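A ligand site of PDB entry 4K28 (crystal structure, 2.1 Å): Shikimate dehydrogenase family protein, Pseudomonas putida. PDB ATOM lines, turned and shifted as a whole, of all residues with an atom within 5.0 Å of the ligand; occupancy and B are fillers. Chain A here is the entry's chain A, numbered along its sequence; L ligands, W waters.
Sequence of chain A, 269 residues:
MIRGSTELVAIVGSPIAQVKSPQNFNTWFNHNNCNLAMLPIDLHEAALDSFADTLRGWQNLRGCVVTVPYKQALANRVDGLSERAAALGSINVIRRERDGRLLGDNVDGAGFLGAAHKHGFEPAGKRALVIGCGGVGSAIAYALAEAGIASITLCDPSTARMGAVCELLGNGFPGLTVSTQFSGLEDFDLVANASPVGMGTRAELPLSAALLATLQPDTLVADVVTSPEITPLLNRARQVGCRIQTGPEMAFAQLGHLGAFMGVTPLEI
Ile 131 touches the ligand (CG2 to C9, 3.3 Å). Cys 133 touches the ligand (C to O5, 3.9 Å). Gly 134 touches the ligand. Cys 155 touches the ligand. CD of Pro 157 touches C10 of the ligand, 3.3 Å away. Ala 194 touches the ligand (O to C11, 3.6 Å). Ser 195 touches the ligand (CB to C10, 3.6 Å). CD of Pro 196 touches O4 of the ligand, at 3.6 Å. CG2 of Val 197 touches N3 of the ligand, at 3.8 Å. Thr 226 touches the ligand (CG2 to N7, 3.7 Å). Met 250 touches the ligand (CG to O14, 3.6 Å). Hydrophobic or aromatic side chains that line the ligand: Ile 131, Val 136, Pro 157, Pro 196, Val 197, Met 199, Val 224, Met 250 and Ala 251. Within 4 Å of the ligand: Ile 131, Gly 132, Cys 133, Gly 134, Gly 135, Val 136, Cys 155, Asp 156, Pro 157, Arg 161, Ala 194, Ser 195, Pro 196, Val 197, Met 199, Val 224, Thr 226, Gly 247, Met 250, Ala 251 and Gln 254.
The backbone NH (N) of Cys 133 sits at hydrogen-bond distance from the side-chain carboxylate (OD2) of Asp 156 (2.7 Å). N of Ser 158 sits at hydrogen-bond distance from OD1 of Asp 156, at 2.8 Å. The backbone NH of Arg 161 lies within hydrogen-bond range of the side-chain hydroxyl of Ser 158 (3.1 Å). The backbone NH of Gly 247 lies close to the backbone carbonyl oxygen of Val 225 (3.4 Å). The backbone NH (N) of Ser 195 lies within hydrogen-bond range of the backbone carbonyl oxygen (O) of Ile 131 (3.3 Å). The backbone NH (N) of Ala 194 is in hydrogen-bond range of the backbone carbonyl oxygen (O) of Ile 131 (2.6 Å). The side-chain amide oxygen of Gln 254 sits close to the side-chain carboxylate of Asp 108 (2.9 Å). The side-chain hydroxyl (OG) of Ser 195 lies close to the backbone NH (N) of Val 197 (3.2 Å).
OD2 of Asp 156 sits at hydrogen-bond distance from O5 of the ligand, 2.7 Å away. An oxygen (O5) of the ligand lies within hydrogen-bond range of the guanidinium group (NE) of Arg 161 (2.7 Å). N of Val 136 is in hydrogen-bond range of O9 of the ligand (2.9 Å). O of Val 224 sits close to N7 of the ligand, 3.0 Å away. N7 of the ligand sits at hydrogen-bond distance from O of Gly 247, at 3.0 Å. An oxygen (O2) of the ligand sits at hydrogen-bond distance from the backbone NH (N) of Gly 135, 3.3 Å away. N of Gly 132 lies close to N5 of the ligand, at 3.5 Å. SD of Met 199 is in hydrogen-bond range of O12 of the ligand (3.4 Å). An oxygen (O14) of the ligand lies close to the backbone NH (N) of Ala 251 (3.5 Å). NE2 of Gln 254 is in hydrogen-bond range of O14 of the ligand, at 3.5 Å.
Water W4 lies within hydrogen-bond range of the backbone carbonyl oxygen of Ala 194 (2.7 Å), the backbone NH of Gly 134 (2.8 Å), the backbone NH of Gly 137 (2.9 Å) and an oxygen (O9) of the ligand (3.0 Å). Water W6 lies within hydrogen-bond range of an oxygen (O13) of the ligand and the backbone NH (N) of Thr 226.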
ATOM      1  N   LYS A  71       7.354  -5.486  20.552  1.00  0.00           N
ATOM      2  CA  LYS A  71       7.877  -5.917  19.258  1.00  0.00           C
ATOM      3  C   LYS A  71       9.240  -6.607  19.370  1.00  0.00           C
ATOM      4  O   LYS A  71       9.464  -7.644  18.756  1.00  0.00           O
ATOM      5  CB  LYS A  71       7.935  -4.751  18.286  1.00  0.00           C
ATOM      6  CG  LYS A  71       6.591  -4.158  17.961  1.00  0.00           C
ATOM      7  CD  LYS A  71       6.704  -3.291  16.709  1.00  0.00           C
ATOM      8  CE  LYS A  71       5.619  -2.251  16.656  1.00  0.00           C
ATOM      9  NZ  LYS A  71       5.563  -1.554  15.335  1.00  0.00           N
ATOM     10  N   ASP A 108       6.087  -3.902   9.030  1.00  0.00           N
ATOM     11  CA  ASP A 108       5.968  -2.452   8.983  1.00  0.00           C
ATOM     12  C   ASP A 108       6.518  -1.950   7.662  1.00  0.00           C
ATOM     13  O   ASP A 108       5.945  -1.057   7.041  1.00  0.00           O
ATOM     14  CB  ASP A 108       6.682  -1.766  10.145  1.00  0.00           C
ATOM     15  CG  ASP A 108       5.823  -1.687  11.411  1.00  0.00           C
ATOM     16  OD1 ASP A 108       4.593  -1.657  11.277  1.00  0.00           O
ATOM     17  OD2 ASP A 108       6.379  -1.676  12.529  1.00  0.00           O
ATOM     18  N   ILE A 131      13.846   9.857   8.360  1.00  0.00           N
ATOM     19  CA  ILE A 131      13.991  10.648   9.578  1.00  0.00           C
ATOM     20  C   ILE A 131      13.498   9.826  10.774  1.00  0.00           C
ATOM     21  O   ILE A 131      12.285   9.654  10.949  1.00  0.00           O
ATOM     22  CB  ILE A 131      13.118  11.926   9.489  1.00  0.00           C
ATOM     23  CG1 ILE A 131      13.454  12.728   8.230  1.00  0.00           C
ATOM     24  CG2 ILE A 131      13.273  12.748  10.736  1.00  0.00           C
ATOM     25  CD1 ILE A 131      12.441  13.816   7.877  1.00  0.00           C
ATOM     26  N   GLY A 132      14.421   9.317  11.591  1.00  0.00           N
ATOM     27  CA  GLY A 132      14.047   8.416  12.670  1.00  0.00           C
ATOM     28  C   GLY A 132      14.599   7.021  12.459  1.00  0.00           C
ATOM     29  O   GLY A 132      14.169   6.288  11.563  1.00  0.00           O
ATOM     30  N   CYS A 133      15.572   6.655  13.277  1.00  0.00           N
ATOM     31  CA  CYS A 133      16.204   5.358  13.106  1.00  0.00           C
ATOM     32  C   CYS A 133      15.732   4.333  14.134  1.00  0.00           C
ATOM     33  O   CYS A 133      16.499   3.459  14.540  1.00  0.00           O
ATOM     34  CB  CYS A 133      17.717   5.514  13.126  1.00  0.00           C
ATOM     35  SG  CYS A 133      18.351   6.261  11.630  1.00  0.00           S
ATOM     36  N   GLY A 134      14.456   4.433  14.515  1.00  0.00           N
ATOM     37  CA  GLY A 134      13.910   3.542  15.515  1.00  0.00           C
ATOM     38  C   GLY A 134      13.411   2.227  14.962  1.00  0.00           C
ATOM     39  O   GLY A 134      13.850   1.759  13.915  1.00  0.00           O
ATOM     40  N   GLY A 135      12.466   1.615  15.665  1.00  0.00           N
ATOM     41  CA  GLY A 135      11.901   0.354  15.225  1.00  0.00           C
ATOM     42  C   GLY A 135      11.217   0.475  13.895  1.00  0.00           C
ATOM     43  O   GLY A 135      11.404  -0.358  13.008  1.00  0.00           O
ATOM     44  N   VAL A 136      10.400   1.508  13.736  1.00  0.00           N
ATOM     45  CA  VAL A 136       9.694   1.681  12.483  1.00  0.00           C
ATOM     46  C   VAL A 136      10.635   2.203  11.397  1.00  0.00           C
ATOM     47  O   VAL A 136      10.568   1.794  10.243  1.00  0.00           O
ATOM     48  CB  VAL A 136       8.497   2.595  12.658  1.00  0.00           C
ATOM     49  CG1 VAL A 136       7.736   2.724  11.360  1.00  0.00           C
ATOM     50  CG2 VAL A 136       7.603   2.028  13.756  1.00  0.00           C
ATOM     51  N   GLY A 137      11.515   3.115  11.778  1.00  0.00           N
ATOM     52  CA  GLY A 137      12.467   3.667  10.824  1.00  0.00           C
ATOM     53  C   GLY A 137      13.394   2.623  10.228  1.00  0.00           C
ATOM     54  O   GLY A 137      13.681   2.651   9.028  1.00  0.00           O
ATOM     55  N   CYS A 155      18.529  10.325   9.428  1.00  0.00           N
ATOM     56  CA  CYS A 155      18.612  11.374  10.459  1.00  0.00           C
ATOM     57  C   CYS A 155      18.034  10.876  11.789  1.00  0.00           C
ATOM     58  O   CYS A 155      16.980  10.255  11.821  1.00  0.00           O
ATOM     59  CB  CYS A 155      17.945  12.697  10.004  1.00  0.00           C
ATOM     60  SG  CYS A 155      17.703  13.935  11.355  1.00  0.00           S
ATOM     61  N   ASP A 156      18.764  11.100  12.873  1.00  0.00           N
ATOM     62  CA  ASP A 156      18.296  10.737  14.199  1.00  0.00           C
ATOM     63  C   ASP A 156      19.235  11.377  15.213  1.00  0.00           C
ATOM     64  O   ASP A 156      20.451  11.241  15.101  1.00  0.00           O
ATOM     65  CB  ASP A 156      18.251   9.213  14.389  1.00  0.00           C
ATOM     66  CG  ASP A 156      17.416   8.785  15.618  1.00  0.00           C
ATOM     67  OD1 ASP A 156      17.554   9.388  16.709  1.00  0.00           O
ATOM     68  OD2 ASP A 156      16.615   7.825  15.492  1.00  0.00           O
ATOM     69  N   PRO A 157      18.672  12.057  16.208  1.00  0.00           N
ATOM     70  CA  PRO A 157      19.509  12.672  17.253  1.00  0.00           C
ATOM     71  C   PRO A 157      20.289  11.590  18.013  1.00  0.00           C
ATOM     72  O   PRO A 157      21.346  11.862  18.568  1.00  0.00           O
ATOM     73  CB  PRO A 157      18.482  13.326  18.175  1.00  0.00           C
ATOM     74  CG  PRO A 157      17.237  13.508  17.306  1.00  0.00           C
ATOM     75  CD  PRO A 157      17.237  12.339  16.383  1.00  0.00           C
ATOM     76  N   SER A 158      19.774  10.367  18.004  1.00  0.00           N
ATOM     77  CA  SER A 158      20.467   9.261  18.642  1.00  0.00           C
ATOM     78  C   SER A 158      21.579   8.733  17.730  1.00  0.00           C
ATOM     79  O   SER A 158      21.330   8.079  16.708  1.00  0.00           O
ATOM     80  CB  SER A 158      19.511   8.155  19.015  1.00  0.00           C
ATOM     81  OG  SER A 158      20.239   6.992  19.357  1.00  0.00           O
ATOM     82  N   ARG A 161      21.650   4.930  17.563  1.00  0.00           N
ATOM     83  CA  ARG A 161      20.662   4.250  16.710  1.00  0.00           C
ATOM     84  C   ARG A 161      20.914   4.528  15.246  1.00  0.00           C
ATOM     85  O   ARG A 161      20.687   3.644  14.396  1.00  0.00           O
ATOM     86  CB  ARG A 161      19.220   4.591  17.113  1.00  0.00           C
ATOM     87  CG  ARG A 161      18.775   3.843  18.386  1.00  0.00           C
ATOM     88  CD  ARG A 161      17.284   3.983  18.659  1.00  0.00           C
ATOM     89  NE  ARG A 161      16.913   5.359  19.013  1.00  0.00           N
ATOM     90  CZ  ARG A 161      17.025   5.887  20.241  1.00  0.00           C
ATOM     91  NH1 ARG A 161      17.502   5.154  21.236  1.00  0.00           N
ATOM     92  NH2 ARG A 161      16.662   7.147  20.474  1.00  0.00           N
ATOM     93  N   ALA A 194       9.859   8.898  10.243  1.00  0.00           N
ATOM     94  CA  ALA A 194       9.574   7.705  11.054  1.00  0.00           C
ATOM     95  C   ALA A 194       9.799   7.978  12.536  1.00  0.00           C
ATOM     96  O   ALA A 194      10.132   7.069  13.283  1.00  0.00           O
ATOM     97  CB  ALA A 194      10.436   6.507  10.625  1.00  0.00           C
ATOM     98  N   SER A 195       9.638   9.245  12.936  1.00  0.00           N
ATOM     99  CA  SER A 195       9.862   9.643  14.322  1.00  0.00           C
ATOM    100  C   SER A 195       8.541  10.004  14.978  1.00  0.00           C
ATOM    101  O   SER A 195       7.524  10.102  14.292  1.00  0.00           O
ATOM    102  CB  SER A 195      10.818  10.844  14.363  1.00  0.00           C
ATOM    103  OG  SER A 195      10.171  12.036  13.923  1.00  0.00           O
ATOM    104  N   PRO A 196       8.533  10.208  16.298  1.00  0.00           N
ATOM    105  CA  PRO A 196       7.305  10.627  16.988  1.00  0.00           C
ATOM    106  C   PRO A 196       6.999  12.078  16.688  1.00  0.00           C
ATOM    107  O   PRO A 196       5.886  12.536  16.973  1.00  0.00           O
ATOM    108  CB  PRO A 196       7.672  10.517  18.469  1.00  0.00           C
ATOM    109  CG  PRO A 196       9.024   9.873  18.529  1.00  0.00           C
ATOM    110  CD  PRO A 196       9.679  10.102  17.225  1.00  0.00           C
ATOM    111  N   VAL A 197       7.957  12.797  16.128  1.00  0.00           N
ATOM    112  CA  VAL A 197       7.732  14.221  15.838  1.00  0.00           C
ATOM    113  C   VAL A 197       6.639  14.388  14.779  1.00  0.00           C
ATOM    114  O   VAL A 197       6.711  13.827  13.677  1.00  0.00           O
ATOM    115  CB  VAL A 197       9.033  14.939  15.386  1.00  0.00           C
ATOM    116  CG1 VAL A 197       8.780  16.424  15.257  1.00  0.00           C
ATOM    117  CG2 VAL A 197      10.159  14.682  16.385  1.00  0.00           C
ATOM    118  N   MET A 199       3.304  14.037  16.057  1.00  0.00           N
ATOM    119  CA  MET A 199       2.183  13.506  16.827  1.00  0.00           C
ATOM    120  C   MET A 199       1.455  14.565  17.666  1.00  0.00           C
ATOM    121  O   MET A 199       2.072  15.468  18.240  1.00  0.00           O
ATOM    122  CB  MET A 199       2.657  12.451  17.819  1.00  0.00           C
ATOM    123  CG  MET A 199       3.212  11.155  17.249  1.00  0.00           C
ATOM    124  SD  MET A 199       3.637  10.023  18.607  1.00  0.00           S
ATOM    125  CE  MET A 199       1.999   9.494  19.079  1.00  0.00           C
ATOM    126  N   PRO A 206       9.889  17.797  12.300  1.00  0.00           N
ATOM    127  CA  PRO A 206      11.202  17.175  12.506  1.00  0.00           C
ATOM    128  C   PRO A 206      12.345  17.874  11.739  1.00  0.00           C
ATOM    129  O   PRO A 206      13.503  17.603  12.030  1.00  0.00           O
ATOM    130  CB  PRO A 206      10.993  15.752  11.967  1.00  0.00           C
ATOM    131  CG  PRO A 206       9.938  15.897  10.977  1.00  0.00           C
ATOM    132  CD  PRO A 206       9.019  16.962  11.468  1.00  0.00           C
ATOM    133  N   VAL A 224       4.678   8.421   9.344  1.00  0.00           N
ATOM    134  CA  VAL A 224       4.160   7.253  10.044  1.00  0.00           C
ATOM    135  C   VAL A 224       3.159   7.652  11.114  1.00  0.00           C
ATOM    136  O   VAL A 224       2.426   6.806  11.619  1.00  0.00           O
ATOM    137  CB  VAL A 224       5.301   6.458  10.739  1.00  0.00           C
ATOM    138  CG1 VAL A 224       6.347   6.053   9.714  1.00  0.00           C
ATOM    139  CG2 VAL A 224       5.913   7.290  11.844  1.00  0.00           C
ATOM    140  N   VAL A 225       3.161   8.926  11.494  1.00  0.00           N
ATOM    141  CA  VAL A 225       2.294   9.393  12.556  1.00  0.00           C
ATOM    142  C   VAL A 225       0.817   9.188  12.203  1.00  0.00           C
ATOM    143  O   VAL A 225       0.397   9.469  11.090  1.00  0.00           O
ATOM    144  CB  VAL A 225       2.518  10.884  12.842  1.00  0.00           C
ATOM    145  CG1 VAL A 225       1.365  11.424  13.664  1.00  0.00           C
ATOM    146  CG2 VAL A 225       3.861  11.099  13.564  1.00  0.00           C
ATOM    147  N   THR A 226       0.030   8.689  13.146  1.00  0.00           N
ATOM    148  CA  THR A 226      -1.367   8.430  12.868  1.00  0.00           C
ATOM    149  C   THR A 226      -2.330   9.507  13.381  1.00  0.00           C
ATOM    150  O   THR A 226      -3.431   9.627  12.856  1.00  0.00           O
ATOM    151  CB  THR A 226      -1.808   7.039  13.376  1.00  0.00           C
ATOM    152  OG1 THR A 226      -1.456   6.872  14.754  1.00  0.00           O
ATOM    153  CG2 THR A 226      -1.123   5.934  12.532  1.00  0.00           C
ATOM    154  N   GLY A 247       0.201   8.275   7.904  1.00  0.00           N
ATOM    155  CA  GLY A 247       0.316   7.154   8.825  1.00  0.00           C
ATOM    156  C   GLY A 247      -0.833   6.175   8.710  1.00  0.00           C
ATOM    157  O   GLY A 247      -0.609   4.965   8.649  1.00  0.00           O
ATOM    158  N   PRO A 248      -2.075   6.668   8.689  1.00  0.00           N
ATOM    159  CA  PRO A 248      -3.191   5.735   8.528  1.00  0.00           C
ATOM    160  C   PRO A 248      -3.093   4.920   7.232  1.00  0.00           C
ATOM    161  O   PRO A 248      -3.475   3.745   7.245  1.00  0.00           O
ATOM    162  CB  PRO A 248      -4.414   6.645   8.511  1.00  0.00           C
ATOM    163  CG  PRO A 248      -3.998   7.815   9.357  1.00  0.00           C
ATOM    164  CD  PRO A 248      -2.565   8.039   8.968  1.00  0.00           C
ATOM    165  N   MET A 250      -0.322   3.870   5.705  1.00  0.00           N
ATOM    166  CA  MET A 250       0.639   2.824   5.989  1.00  0.00           C
ATOM    167  C   MET A 250       0.061   1.748   6.884  1.00  0.00           C
ATOM    168  O   MET A 250       0.235   0.568   6.633  1.00  0.00           O
ATOM    169  CB  MET A 250       1.879   3.407   6.653  1.00  0.00           C
ATOM    170  CG  MET A 250       2.769   2.336   7.254  1.00  0.00           C
ATOM    171  SD  MET A 250       4.215   3.103   7.977  1.00  0.00           S
ATOM    172  CE  MET A 250       4.986   1.706   8.773  1.00  0.00           C
ATOM    173  N   ALA A 251      -0.621   2.148   7.958  1.00  0.00           N
ATOM    174  CA  ALA A 251      -1.225   1.152   8.851  1.00  0.00           C
ATOM    175  C   ALA A 251      -2.206   0.256   8.102  1.00  0.00           C
ATOM    176  O   ALA A 251      -2.217  -0.963   8.270  1.00  0.00           O
ATOM    177  CB  ALA A 251      -1.904   1.828  10.023  1.00  0.00           C
ATOM    178  N   GLN A 254      -0.931  -2.394   5.759  1.00  0.00           N
ATOM    179  CA  GLN A 254      -0.337  -3.524   6.463  1.00  0.00           C
ATOM    180  C   GLN A 254      -1.387  -4.605   6.741  1.00  0.00           C
ATOM    181  O   GLN A 254      -1.168  -5.778   6.440  1.00  0.00           O
ATOM    182  CB  GLN A 254       0.301  -3.067   7.775  1.00  0.00           C
ATOM    183  CG  GLN A 254       1.722  -2.558   7.623  1.00  0.00           C
ATOM    184  CD  GLN A 254       2.368  -2.225   8.954  1.00  0.00           C
ATOM    185  OE1 GLN A 254       2.532  -3.097   9.808  1.00  0.00           O
ATOM    186  NE2 GLN A 254       2.739  -0.960   9.137  1.00  0.00           N
HETATM  187  P1  LIG L   1      11.045   4.552  18.286  1.00  0.00           P
HETATM  188  O1  LIG L   1      11.165   5.215  19.453  1.00  0.00           O
HETATM  189  O2  LIG L   1      11.499   3.229  18.340  1.00  0.00           O
HETATM  190  O3  LIG L   1      11.866   5.243  17.300  1.00  0.00           O
HETATM  191  C1  LIG L   1      11.764   6.552  17.032  1.00  0.00           C
HETATM  192  C2  LIG L   1      13.047   7.184  16.632  1.00  0.00           C
HETATM  193  O4  LIG L   1      12.824   8.520  16.381  1.00  0.00           O
HETATM  194  C3  LIG L   1      14.071   7.123  17.764  1.00  0.00           C
HETATM  195  O5  LIG L   1      15.202   6.518  17.316  1.00  0.00           O
HETATM  196  C4  LIG L   1      14.274   8.600  18.011  1.00  0.00           C
HETATM  197  O6  LIG L   1      15.545   8.852  18.394  1.00  0.00           O
HETATM  198  C5  LIG L   1      13.923   9.178  16.619  1.00  0.00           C
HETATM  199  N1  LIG L   1      13.780  10.660  16.552  1.00  0.00           N
HETATM  200  C6  LIG L   1      13.267  11.399  17.483  1.00  0.00           C
HETATM  201  N2  LIG L   1      13.309  12.622  17.157  1.00  0.00           N
HETATM  202  C7  LIG L   1      13.798  12.709  15.971  1.00  0.00           C
HETATM  203  C8  LIG L   1      14.064  13.739  15.111  1.00  0.00           C
HETATM  204  N3  LIG L   1      13.807  14.986  15.407  1.00  0.00           N
HETATM  205  N4  LIG L   1      14.616  13.498  13.975  1.00  0.00           N
HETATM  206  C9  LIG L   1      14.887  12.306  13.634  1.00  0.00           C
HETATM  207  N5  LIG L   1      14.653  11.309  14.419  1.00  0.00           N
HETATM  208  C10 LIG L   1      14.111  11.460  15.599  1.00  0.00           C
HETATM  209  O7  LIG L   1       9.578   4.457  17.848  1.00  0.00           O
HETATM  210  P2  LIG L   1       8.938   3.739  16.728  1.00  0.00           P
HETATM  211  O8  LIG L   1       8.359   2.656  17.171  1.00  0.00           O
HETATM  212  O9  LIG L   1       9.735   3.627  15.627  1.00  0.00           O
HETATM  213  O10 LIG L   1       7.831   4.496  16.288  1.00  0.00           O
HETATM  214  C11 LIG L   1       7.895   5.809  15.842  1.00  0.00           C
HETATM  215  C12 LIG L   1       6.608   6.460  15.354  1.00  0.00           C
HETATM  216  O11 LIG L   1       6.015   5.643  14.378  1.00  0.00           O
HETATM  217  C13 LIG L   1       5.537   6.691  16.422  1.00  0.00           C
HETATM  218  O12 LIG L   1       4.818   7.871  16.204  1.00  0.00           O
HETATM  219  C14 LIG L   1       4.644   5.504  16.132  1.00  0.00           C
HETATM  220  O13 LIG L   1       3.428   5.745  16.666  1.00  0.00           O
HETATM  221  C15 LIG L   1       4.633   5.517  14.645  1.00  0.00           C
HETATM  222  N6  LIG L   1       4.188   4.295  13.939  1.00  0.00           N
HETATM  223  C16 LIG L   1       3.283   4.314  12.872  1.00  0.00           C
HETATM  224  C17 LIG L   1       2.897   3.136  12.225  1.00  0.00           C
HETATM  225  C18 LIG L   1       1.939   3.072  11.058  1.00  0.00           C
HETATM  226  O14 LIG L   1       1.604   1.999  10.617  1.00  0.00           O
HETATM  227  N7  LIG L   1       1.539   4.194  10.568  1.00  0.00           N
HETATM  228  C19 LIG L   1       3.437   1.936  12.608  1.00  0.00           C
HETATM  229  C20 LIG L   1       4.318   1.915  13.653  1.00  0.00           C
HETATM  230  C21 LIG L   1       4.682   3.082  14.306  1.00  0.00           C
HETATM  231  O   HOH W   1      14.023   2.372  19.394  1.00  0.00           O
HETATM  232  O   HOH W   2      13.141  17.202  17.245  1.00  0.00           O
HETATM  233  O   HOH W   3      12.314  14.295  19.711  1.00  0.00           O
HETATM  234  O   HOH W   4      11.812   5.068  13.931  1.00  0.00           O
HETATM  235  O   HOH W   5      10.521   0.653  19.374  1.00  0.00           O
HETATM  236  O   HOH W   6       1.433   8.078  16.003  1.00  0.00           O
HETATM  237  O   HOH W   7      15.996  11.147  20.601  1.00  0.00           O
